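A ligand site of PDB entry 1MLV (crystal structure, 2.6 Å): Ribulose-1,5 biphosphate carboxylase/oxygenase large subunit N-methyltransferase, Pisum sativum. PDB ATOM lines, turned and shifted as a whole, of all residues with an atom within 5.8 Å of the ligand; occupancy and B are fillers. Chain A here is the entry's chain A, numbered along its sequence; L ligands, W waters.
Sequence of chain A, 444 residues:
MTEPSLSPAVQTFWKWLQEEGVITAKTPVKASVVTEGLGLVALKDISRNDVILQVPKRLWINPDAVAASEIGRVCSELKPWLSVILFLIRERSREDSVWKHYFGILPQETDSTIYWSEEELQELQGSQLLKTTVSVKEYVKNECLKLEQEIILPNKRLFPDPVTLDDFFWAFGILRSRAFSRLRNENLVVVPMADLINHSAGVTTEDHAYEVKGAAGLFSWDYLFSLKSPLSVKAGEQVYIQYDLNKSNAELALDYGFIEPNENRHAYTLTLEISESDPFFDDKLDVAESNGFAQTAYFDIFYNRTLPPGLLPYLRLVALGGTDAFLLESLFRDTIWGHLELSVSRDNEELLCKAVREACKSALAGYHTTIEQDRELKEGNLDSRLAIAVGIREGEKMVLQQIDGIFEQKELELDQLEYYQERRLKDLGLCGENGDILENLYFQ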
ATOM      1  N   VAL A  34       4.619   5.260   1.762  1.00  0.00           N
ATOM      2  CA  VAL A  34       4.377   5.358   0.336  1.00  0.00           C
ATOM      3  C   VAL A  34       3.740   6.705  -0.004  1.00  0.00           C
ATOM      4  O   VAL A  34       3.280   7.405   0.897  1.00  0.00           O
ATOM      5  CB  VAL A  34       3.463   4.221  -0.139  1.00  0.00           C
ATOM      6  CG1 VAL A  34       4.147   2.882   0.057  1.00  0.00           C
ATOM      7  CG2 VAL A  34       2.152   4.266   0.637  1.00  0.00           C
ATOM      8  N   GLU A  36       1.044   7.431  -0.813  1.00  0.00           N
ATOM      9  CA  GLU A  36      -0.270   7.519  -0.197  1.00  0.00           C
ATOM     10  C   GLU A  36      -0.253   7.355   1.335  1.00  0.00           C
ATOM     11  O   GLU A  36      -1.241   6.902   1.916  1.00  0.00           O
ATOM     12  CB  GLU A  36      -1.229   6.506  -0.817  1.00  0.00           C
ATOM     13  CG  GLU A  36      -0.669   5.119  -0.946  1.00  0.00           C
ATOM     14  CD  GLU A  36       0.133   4.918  -2.221  1.00  0.00           C
ATOM     15  OE1 GLU A  36      -0.482   4.557  -3.243  1.00  0.00           O
ATOM     16  OE2 GLU A  36       1.376   5.145  -2.192  1.00  0.00           O
ATOM     17  N   GLY A  37       0.856   7.730   1.960  1.00  0.00           N
ATOM     18  CA  GLY A  37       0.972   7.640   3.401  1.00  0.00           C
ATOM     19  C   GLY A  37       1.640   6.385   3.918  1.00  0.00           C
ATOM     20  O   GLY A  37       2.842   6.179   3.735  1.00  0.00           O
ATOM     21  N   LEU A  38       0.865   5.542   4.577  1.00  0.00           N
ATOM     22  CA  LEU A  38       1.368   4.281   5.109  1.00  0.00           C
ATOM     23  C   LEU A  38       0.799   3.180   4.239  1.00  0.00           C
ATOM     24  O   LEU A  38      -0.336   3.269   3.796  1.00  0.00           O
ATOM     25  CB  LEU A  38       0.920   4.092   6.545  1.00  0.00           C
ATOM     26  CG  LEU A  38       1.922   4.476   7.635  1.00  0.00           C
ATOM     27  CD1 LEU A  38       1.233   4.496   8.989  1.00  0.00           C
ATOM     28  CD2 LEU A  38       3.082   3.468   7.605  1.00  0.00           C
ATOM     29  N   GLY A  39       1.589   2.146   3.999  1.00  0.00           N
ATOM     30  CA  GLY A  39       1.100   1.058   3.180  1.00  0.00           C
ATOM     31  C   GLY A  39       1.816  -0.254   3.429  1.00  0.00           C
ATOM     32  O   GLY A  39       2.792  -0.307   4.174  1.00  0.00           O
ATOM     33  N   ILE A 105      -1.109   5.722  15.518  1.00  0.00           N
ATOM     34  CA  ILE A 105      -0.758   5.634  14.089  1.00  0.00           C
ATOM     35  C   ILE A 105      -1.801   6.292  13.188  1.00  0.00           C
ATOM     36  O   ILE A 105      -1.482   6.778  12.112  1.00  0.00           O
ATOM     37  CB  ILE A 105      -0.573   4.152  13.656  1.00  0.00           C
ATOM     38  CG1 ILE A 105       0.766   3.650  14.160  1.00  0.00           C
ATOM     39  CG2 ILE A 105      -0.580   4.019  12.162  1.00  0.00           C
ATOM     40  CD1 ILE A 105       1.911   4.480  13.674  1.00  0.00           C
ATOM     41  N   PRO A 107      -3.928   8.784  11.251  1.00  0.00           N
ATOM     42  CA  PRO A 107      -3.671  10.153  10.790  1.00  0.00           C
ATOM     43  C   PRO A 107      -4.682  11.074  11.460  1.00  0.00           C
ATOM     44  O   PRO A 107      -5.847  10.711  11.623  1.00  0.00           O
ATOM     45  CB  PRO A 107      -3.886  10.065   9.289  1.00  0.00           C
ATOM     46  CG  PRO A 107      -3.562   8.622   8.975  1.00  0.00           C
ATOM     47  CD  PRO A 107      -4.232   7.904  10.102  1.00  0.00           C
ATOM     48  N   THR A 110      -7.544  13.339   6.902  1.00  0.00           N
ATOM     49  CA  THR A 110      -7.395  12.758   5.568  1.00  0.00           C
ATOM     50  C   THR A 110      -7.703  13.917   4.638  1.00  0.00           C
ATOM     51  O   THR A 110      -7.784  15.062   5.092  1.00  0.00           O
ATOM     52  CB  THR A 110      -8.408  11.635   5.280  1.00  0.00           C
ATOM     53  OG1 THR A 110      -9.733  12.186   5.263  1.00  0.00           O
ATOM     54  CG2 THR A 110      -8.310  10.552   6.331  1.00  0.00           C
ATOM     55  N   ASP A 111      -7.863  13.650   3.348  1.00  0.00           N
ATOM     56  CA  ASP A 111      -8.185  14.740   2.435  1.00  0.00           C
ATOM     57  C   ASP A 111      -9.665  14.773   2.125  1.00  0.00           C
ATOM     58  O   ASP A 111     -10.109  15.451   1.193  1.00  0.00           O
ATOM     59  CB  ASP A 111      -7.354  14.645   1.163  1.00  0.00           C
ATOM     60  CG  ASP A 111      -5.963  15.228   1.343  1.00  0.00           C
ATOM     61  OD1 ASP A 111      -5.868  16.367   1.836  1.00  0.00           O
ATOM     62  OD2 ASP A 111      -4.976  14.548   0.996  1.00  0.00           O
ATOM     63  N   SER A 177     -13.390   6.070   6.273  1.00  0.00           N
ATOM     64  CA  SER A 177     -12.278   5.796   5.386  1.00  0.00           C
ATOM     65  C   SER A 177     -11.456   4.565   5.744  1.00  0.00           C
ATOM     66  O   SER A 177     -10.453   4.306   5.115  1.00  0.00           O
ATOM     67  CB  SER A 177     -11.364   7.020   5.315  1.00  0.00           C
ATOM     68  OG  SER A 177     -10.897   7.426   6.591  1.00  0.00           O
ATOM     69  N   ARG A 178     -11.893   3.799   6.748  1.00  0.00           N
ATOM     70  CA  ARG A 178     -11.145   2.603   7.137  1.00  0.00           C
ATOM     71  C   ARG A 178     -11.949   1.329   7.379  1.00  0.00           C
ATOM     72  O   ARG A 178     -11.518   0.234   7.020  1.00  0.00           O
ATOM     73  CB  ARG A 178     -10.300   2.910   8.377  1.00  0.00           C
ATOM     74  CG  ARG A 178      -9.123   3.776   8.089  1.00  0.00           C
ATOM     75  CD  ARG A 178      -8.461   4.218   9.362  1.00  0.00           C
ATOM     76  NE  ARG A 178      -7.148   4.812   9.093  1.00  0.00           N
ATOM     77  CZ  ARG A 178      -6.017   4.119   8.993  1.00  0.00           C
ATOM     78  NH1 ARG A 178      -6.005   2.804   9.159  1.00  0.00           N
ATOM     79  NH2 ARG A 178      -4.887   4.756   8.711  1.00  0.00           N
ATOM     80  N   ASP A 195      -5.728  -2.837   8.187  1.00  0.00           N
ATOM     81  CA  ASP A 195      -6.262  -1.510   8.012  1.00  0.00           C
ATOM     82  C   ASP A 195      -5.152  -0.588   7.543  1.00  0.00           C
ATOM     83  O   ASP A 195      -5.006   0.537   8.023  1.00  0.00           O
ATOM     84  CB  ASP A 195      -6.855  -1.031   9.346  1.00  0.00           C
ATOM     85  CG  ASP A 195      -7.624   0.254   9.206  1.00  0.00           C
ATOM     86  OD1 ASP A 195      -8.452   0.342   8.271  1.00  0.00           O
ATOM     87  OD2 ASP A 195      -7.413   1.161  10.028  1.00  0.00           O
ATOM     88  N   LEU A 196      -4.374  -1.077   6.579  1.00  0.00           N
ATOM     89  CA  LEU A 196      -3.267  -0.308   6.022  1.00  0.00           C
ATOM     90  C   LEU A 196      -3.205  -0.330   4.499  1.00  0.00           C
ATOM     91  O   LEU A 196      -2.748   0.643   3.894  1.00  0.00           O
ATOM     92  CB  LEU A 196      -1.934  -0.818   6.597  1.00  0.00           C
ATOM     93  CG  LEU A 196      -1.578  -0.443   8.041  1.00  0.00           C
ATOM     94  CD1 LEU A 196      -0.305  -1.161   8.445  1.00  0.00           C
ATOM     95  CD2 LEU A 196      -1.396   1.055   8.143  1.00  0.00           C
ATOM     96  N   ILE A 197      -3.647  -1.418   3.866  1.00  0.00           N
ATOM     97  CA  ILE A 197      -3.614  -1.497   2.400  1.00  0.00           C
ATOM     98  C   ILE A 197      -4.296  -0.281   1.780  1.00  0.00           C
ATOM     99  O   ILE A 197      -5.294   0.234   2.285  1.00  0.00           O
ATOM    100  CB  ILE A 197      -4.325  -2.746   1.827  1.00  0.00           C
ATOM    101  CG1 ILE A 197      -5.502  -3.143   2.718  1.00  0.00           C
ATOM    102  CG2 ILE A 197      -3.351  -3.879   1.633  1.00  0.00           C
ATOM    103  CD1 ILE A 197      -6.635  -2.143   2.700  1.00  0.00           C
ATOM    104  N   ASN A 198      -3.744   0.163   0.656  1.00  0.00           N
ATOM    105  CA  ASN A 198      -4.290   1.295  -0.040  1.00  0.00           C
ATOM    106  C   ASN A 198      -5.055   0.836  -1.276  1.00  0.00           C
ATOM    107  O   ASN A 198      -4.996  -0.333  -1.656  1.00  0.00           O
ATOM    108  CB  ASN A 198      -3.163   2.247  -0.408  1.00  0.00           C
ATOM    109  CG  ASN A 198      -2.504   2.840   0.816  1.00  0.00           C
ATOM    110  OD1 ASN A 198      -3.145   3.530   1.593  1.00  0.00           O
ATOM    111  ND2 ASN A 198      -1.222   2.547   1.000  1.00  0.00           N
ATOM    112  N   HIS A 199      -5.769   1.775  -1.884  1.00  0.00           N
ATOM    113  CA  HIS A 199      -6.563   1.503  -3.076  1.00  0.00           C
ATOM    114  C   HIS A 199      -5.732   1.641  -4.343  1.00  0.00           C
ATOM    115  O   HIS A 199      -4.795   2.436  -4.383  1.00  0.00           O
ATOM    116  CB  HIS A 199      -7.740   2.490  -3.116  1.00  0.00           C
ATOM    117  CG  HIS A 199      -8.451   2.533  -4.426  1.00  0.00           C
ATOM    118  ND1 HIS A 199      -9.475   1.674  -4.746  1.00  0.00           N
ATOM    119  CD2 HIS A 199      -8.252   3.308  -5.523  1.00  0.00           C
ATOM    120  CE1 HIS A 199      -9.893   1.918  -5.980  1.00  0.00           C
ATOM    121  NE2 HIS A 199      -9.169   2.910  -6.472  1.00  0.00           N
ATOM    122  N   SER A 200      -6.059   0.871  -5.377  1.00  0.00           N
ATOM    123  CA  SER A 200      -5.367   0.952  -6.662  1.00  0.00           C
ATOM    124  C   SER A 200      -6.328   0.650  -7.802  1.00  0.00           C
ATOM    125  O   SER A 200      -7.090  -0.310  -7.729  1.00  0.00           O
ATOM    126  CB  SER A 200      -4.216  -0.023  -6.741  1.00  0.00           C
ATOM    127  OG  SER A 200      -3.679  -0.015  -8.051  1.00  0.00           O
ATOM    128  N   TYR A 240      -2.008  -3.851  -3.072  1.00  0.00           N
ATOM    129  CA  TYR A 240      -3.207  -3.008  -3.139  1.00  0.00           C
ATOM    130  C   TYR A 240      -4.523  -3.757  -3.196  1.00  0.00           C
ATOM    131  O   TYR A 240      -4.555  -4.992  -3.285  1.00  0.00           O
ATOM    132  CB  TYR A 240      -3.160  -2.102  -4.394  1.00  0.00           C
ATOM    133  CG  TYR A 240      -2.133  -0.983  -4.394  1.00  0.00           C
ATOM    134  CD1 TYR A 240      -1.002  -1.032  -5.221  1.00  0.00           C
ATOM    135  CD2 TYR A 240      -2.314   0.152  -3.600  1.00  0.00           C
ATOM    136  CE1 TYR A 240      -0.092   0.019  -5.268  1.00  0.00           C
ATOM    137  CE2 TYR A 240      -1.400   1.214  -3.635  1.00  0.00           C
ATOM    138  CZ  TYR A 240      -0.300   1.134  -4.473  1.00  0.00           C
ATOM    139  OH  TYR A 240       0.599   2.181  -4.513  1.00  0.00           O
ATOM    140  N   TYR A 243     -10.972  -0.502  -3.318  1.00  0.00           N
ATOM    141  CA  TYR A 243     -11.926  -0.090  -2.292  1.00  0.00           C
ATOM    142  C   TYR A 243     -13.369  -0.299  -2.725  1.00  0.00           C
ATOM    143  O   TYR A 243     -14.157  -0.867  -1.984  1.00  0.00           O
ATOM    144  CB  TYR A 243     -11.699   1.365  -1.865  1.00  0.00           C
ATOM    145  CG  TYR A 243     -10.492   1.570  -0.956  1.00  0.00           C
ATOM    146  CD1 TYR A 243     -10.212   2.832  -0.413  1.00  0.00           C
ATOM    147  CD2 TYR A 243      -9.618   0.511  -0.673  1.00  0.00           C
ATOM    148  CE1 TYR A 243      -9.081   3.029   0.385  1.00  0.00           C
ATOM    149  CE2 TYR A 243      -8.484   0.700   0.124  1.00  0.00           C
ATOM    150  CZ  TYR A 243      -8.215   1.970   0.655  1.00  0.00           C
ATOM    151  OH  TYR A 243      -7.091   2.166   1.441  1.00  0.00           O
ATOM    152  N   ASP A 255     -15.590   9.808   1.162  1.00  0.00           N
ATOM    153  CA  ASP A 255     -15.338   8.618   1.971  1.00  0.00           C
ATOM    154  C   ASP A 255     -13.867   8.480   2.355  1.00  0.00           C
ATOM    155  O   ASP A 255     -13.538   8.243   3.509  1.00  0.00           O
ATOM    156  CB  ASP A 255     -15.830   7.374   1.229  1.00  0.00           C
ATOM    157  CG  ASP A 255     -17.343   7.214   1.317  1.00  0.00           C
ATOM    158  OD1 ASP A 255     -17.829   6.891   2.412  1.00  0.00           O
ATOM    159  OD2 ASP A 255     -18.055   7.413   0.301  1.00  0.00           O
ATOM    160  N   TYR A 256     -12.980   8.614   1.370  1.00  0.00           N
ATOM    161  CA  TYR A 256     -11.533   8.564   1.618  1.00  0.00           C
ATOM    162  C   TYR A 256     -11.092   9.909   1.068  1.00  0.00           C
ATOM    163  O   TYR A 256     -11.928  10.706   0.638  1.00  0.00           O
ATOM    164  CB  TYR A 256     -10.873   7.425   0.825  1.00  0.00           C
ATOM    165  CG  TYR A 256     -11.761   6.219   0.655  1.00  0.00           C
ATOM    166  CD1 TYR A 256     -12.537   6.056  -0.494  1.00  0.00           C
ATOM    167  CD2 TYR A 256     -11.854   5.265   1.654  1.00  0.00           C
ATOM    168  CE1 TYR A 256     -13.395   4.964  -0.629  1.00  0.00           C
ATOM    169  CE2 TYR A 256     -12.705   4.174   1.532  1.00  0.00           C
ATOM    170  CZ  TYR A 256     -13.480   4.032   0.396  1.00  0.00           C
ATOM    171  OH  TYR A 256     -14.330   2.961   0.287  1.00  0.00           O
ATOM    172  N   GLY A 257      -9.802  10.186   1.065  1.00  0.00           N
ATOM    173  CA  GLY A 257      -9.410  11.470   0.526  1.00  0.00           C
ATOM    174  C   GLY A 257      -8.790  11.374  -0.845  1.00  0.00           C
ATOM    175  O   GLY A 257      -7.663  11.832  -1.021  1.00  0.00           O
ATOM    176  N   PHE A 258      -9.495  10.819  -1.824  1.00  0.00           N
ATOM    177  CA  PHE A 258      -8.931  10.669  -3.164  1.00  0.00           C
ATOM    178  C   PHE A 258      -9.951  10.374  -4.254  1.00  0.00           C
ATOM    179  O   PHE A 258     -11.046   9.897  -3.969  1.00  0.00           O
ATOM    180  CB  PHE A 258      -7.877   9.558  -3.161  1.00  0.00           C
ATOM    181  CG  PHE A 258      -8.452   8.169  -3.146  1.00  0.00           C
ATOM    182  CD1 PHE A 258      -8.960   7.590  -4.303  1.00  0.00           C
ATOM    183  CD2 PHE A 258      -8.452   7.412  -1.961  1.00  0.00           C
ATOM    184  CE1 PHE A 258      -9.469   6.278  -4.302  1.00  0.00           C
ATOM    185  CE2 PHE A 258      -8.966   6.097  -1.941  1.00  0.00           C
ATOM    186  CZ  PHE A 258      -9.470   5.521  -3.117  1.00  0.00           C
HETATM  187  N1  LIG L   1      -2.376   5.150   3.709  1.00  0.00           N
HETATM  188  C1  LIG L   1      -3.192   5.074   4.927  1.00  0.00           C
HETATM  189  C2  LIG L   1      -3.615   3.610   5.191  1.00  0.00           C
HETATM  190  C3  LIG L   1      -4.811   3.154   4.421  1.00  0.00           C
HETATM  191  S1  LIG L   1      -6.431   3.697   5.063  1.00  0.00           S
HETATM  192  C4  LIG L   1      -2.416   5.676   6.147  1.00  0.00           C
HETATM  193  O1  LIG L   1      -2.969   5.711   7.264  1.00  0.00           O
HETATM  194  O2  LIG L   1      -1.259   6.121   5.995  1.00  0.00           O
HETATM  195  C5  LIG L   1      -7.060   4.473   3.577  1.00  0.00           C
HETATM  196  C6  LIG L   1      -6.634   5.908   3.412  1.00  0.00           C
HETATM  197  O3  LIG L   1      -5.317   5.968   2.809  1.00  0.00           O
HETATM  198  C7  LIG L   1      -7.514   6.740   2.501  1.00  0.00           C
HETATM  199  O4  LIG L   1      -8.622   7.308   3.187  1.00  0.00           O
HETATM  200  C8  LIG L   1      -6.558   7.776   1.944  1.00  0.00           C
HETATM  201  O5  LIG L   1      -6.385   8.950   2.707  1.00  0.00           O
HETATM  202  C9  LIG L   1      -5.296   6.923   1.754  1.00  0.00           C
HETATM  203  N2  LIG L   1      -5.257   6.228   0.439  1.00  0.00           N
HETATM  204  C10 LIG L   1      -5.516   4.912   0.121  1.00  0.00           C
HETATM  205  N3  LIG L   1      -5.396   4.635  -1.150  1.00  0.00           N
HETATM  206  C11 LIG L   1      -5.037   5.846  -1.718  1.00  0.00           C
HETATM  207  C12 LIG L   1      -4.767   6.243  -3.067  1.00  0.00           C
HETATM  208  N4  LIG L   1      -4.822   5.396  -4.094  1.00  0.00           N
HETATM  209  N5  LIG L   1      -4.437   7.545  -3.315  1.00  0.00           N
HETATM  210  C13 LIG L   1      -4.379   8.434  -2.270  1.00  0.00           C
HETATM  211  N6  LIG L   1      -4.620   8.178  -0.955  1.00  0.00           N
HETATM  212  C14 LIG L   1      -4.950   6.847  -0.752  1.00  0.00           C
HETATM  213  O   HOH W   1      -6.984  11.317   2.009  1.00  0.00           O
HETATM  214  O   HOH W   2      -2.316   4.127  -5.973  1.00  0.00           O
HETATM  215  O   HOH W   3      -0.270   7.765   7.707  1.00  0.00           O
HETATM  216  O   HOH W   4      -2.234   4.708   9.752  1.00  0.00           O
HETATM  217  O   HOH W   5      -4.372   8.205   4.741  1.00  0.00           O
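The backbone carbonyl oxygen (O) of His 199 lies within hydrogen-bond range of a nitrogen (N4) of the ligand.
A nitrogen (N1) of the ligand sits at hydrogen-bond distance from the side-chain amide oxygen (OD1) of Asn 198, 2.8 Å away.
O of Leu 38 lies within hydrogen-bond range of N1 of the ligand, 2.8 Å away.
A nitrogen (N1) of the ligand sits at hydrogen-bond distance from the backbone carbonyl oxygen (O) of Glu 36 (2.8 Å).
An oxygen (O2) of the ligand sits at hydrogen-bond distance from the backbone NH (N) of Leu 38, 2.6 Å away.
N of His 199 sits at hydrogen-bond distance from N3 of the ligand, 3.0 Å away.
An oxygen (O1) of the ligand lies within salt-bridge range of the guanidinium group (NH2) of Arg 178, 2.6 Å away.
OH of Tyr 243 is in hydrogen-bond range of O of Ile 197 (2.8 Å).
The guanidinium group (NH1) of Arg 178 lies within salt-bridge range of the side-chain carboxylate (OD1) of Asp 195, 3.6 Å away.
A ring nitrogen (ND1) of His 199 sits at hydrogen-bond distance from the backbone NH (N) of Tyr 243 (3.0 Å).
O of Leu 38 lies within hydrogen-bond range of ND2 of Asn 198 (3.0 Å).
OE1 of Glu 36 is in hydrogen-bond range of OH of Tyr 240 (2.9 Å).
Merely in contact with the ligand: Tyr 243, Tyr 256, Leu 196, Pro 107, Ser 177, Gly 37, Ile 197, Phe 258 and Gly 257.
The nearest printed residue that does not touch the ligand is Thr 110 (4.2 Å).
Water W1 lies within hydrogen-bond range of O5 of the ligand (2.5 Å), N of Asp 111 (2.8 Å) and O of Gly 257 (3.1 Å).
Water W4 lies within hydrogen-bond range of an oxygen (O1) of the ligand (2.8 Å), the guanidinium group (NH2) of Arg 178 (2.9 Å) and the backbone carbonyl oxygen (O) of Ile 105 (3.2 Å).
Water W2 lies within hydrogen-bond range of OE1 of Glu 36 (3.3 Å), N4 of the ligand (3.4 Å) and O of His 199 (3.4 Å).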
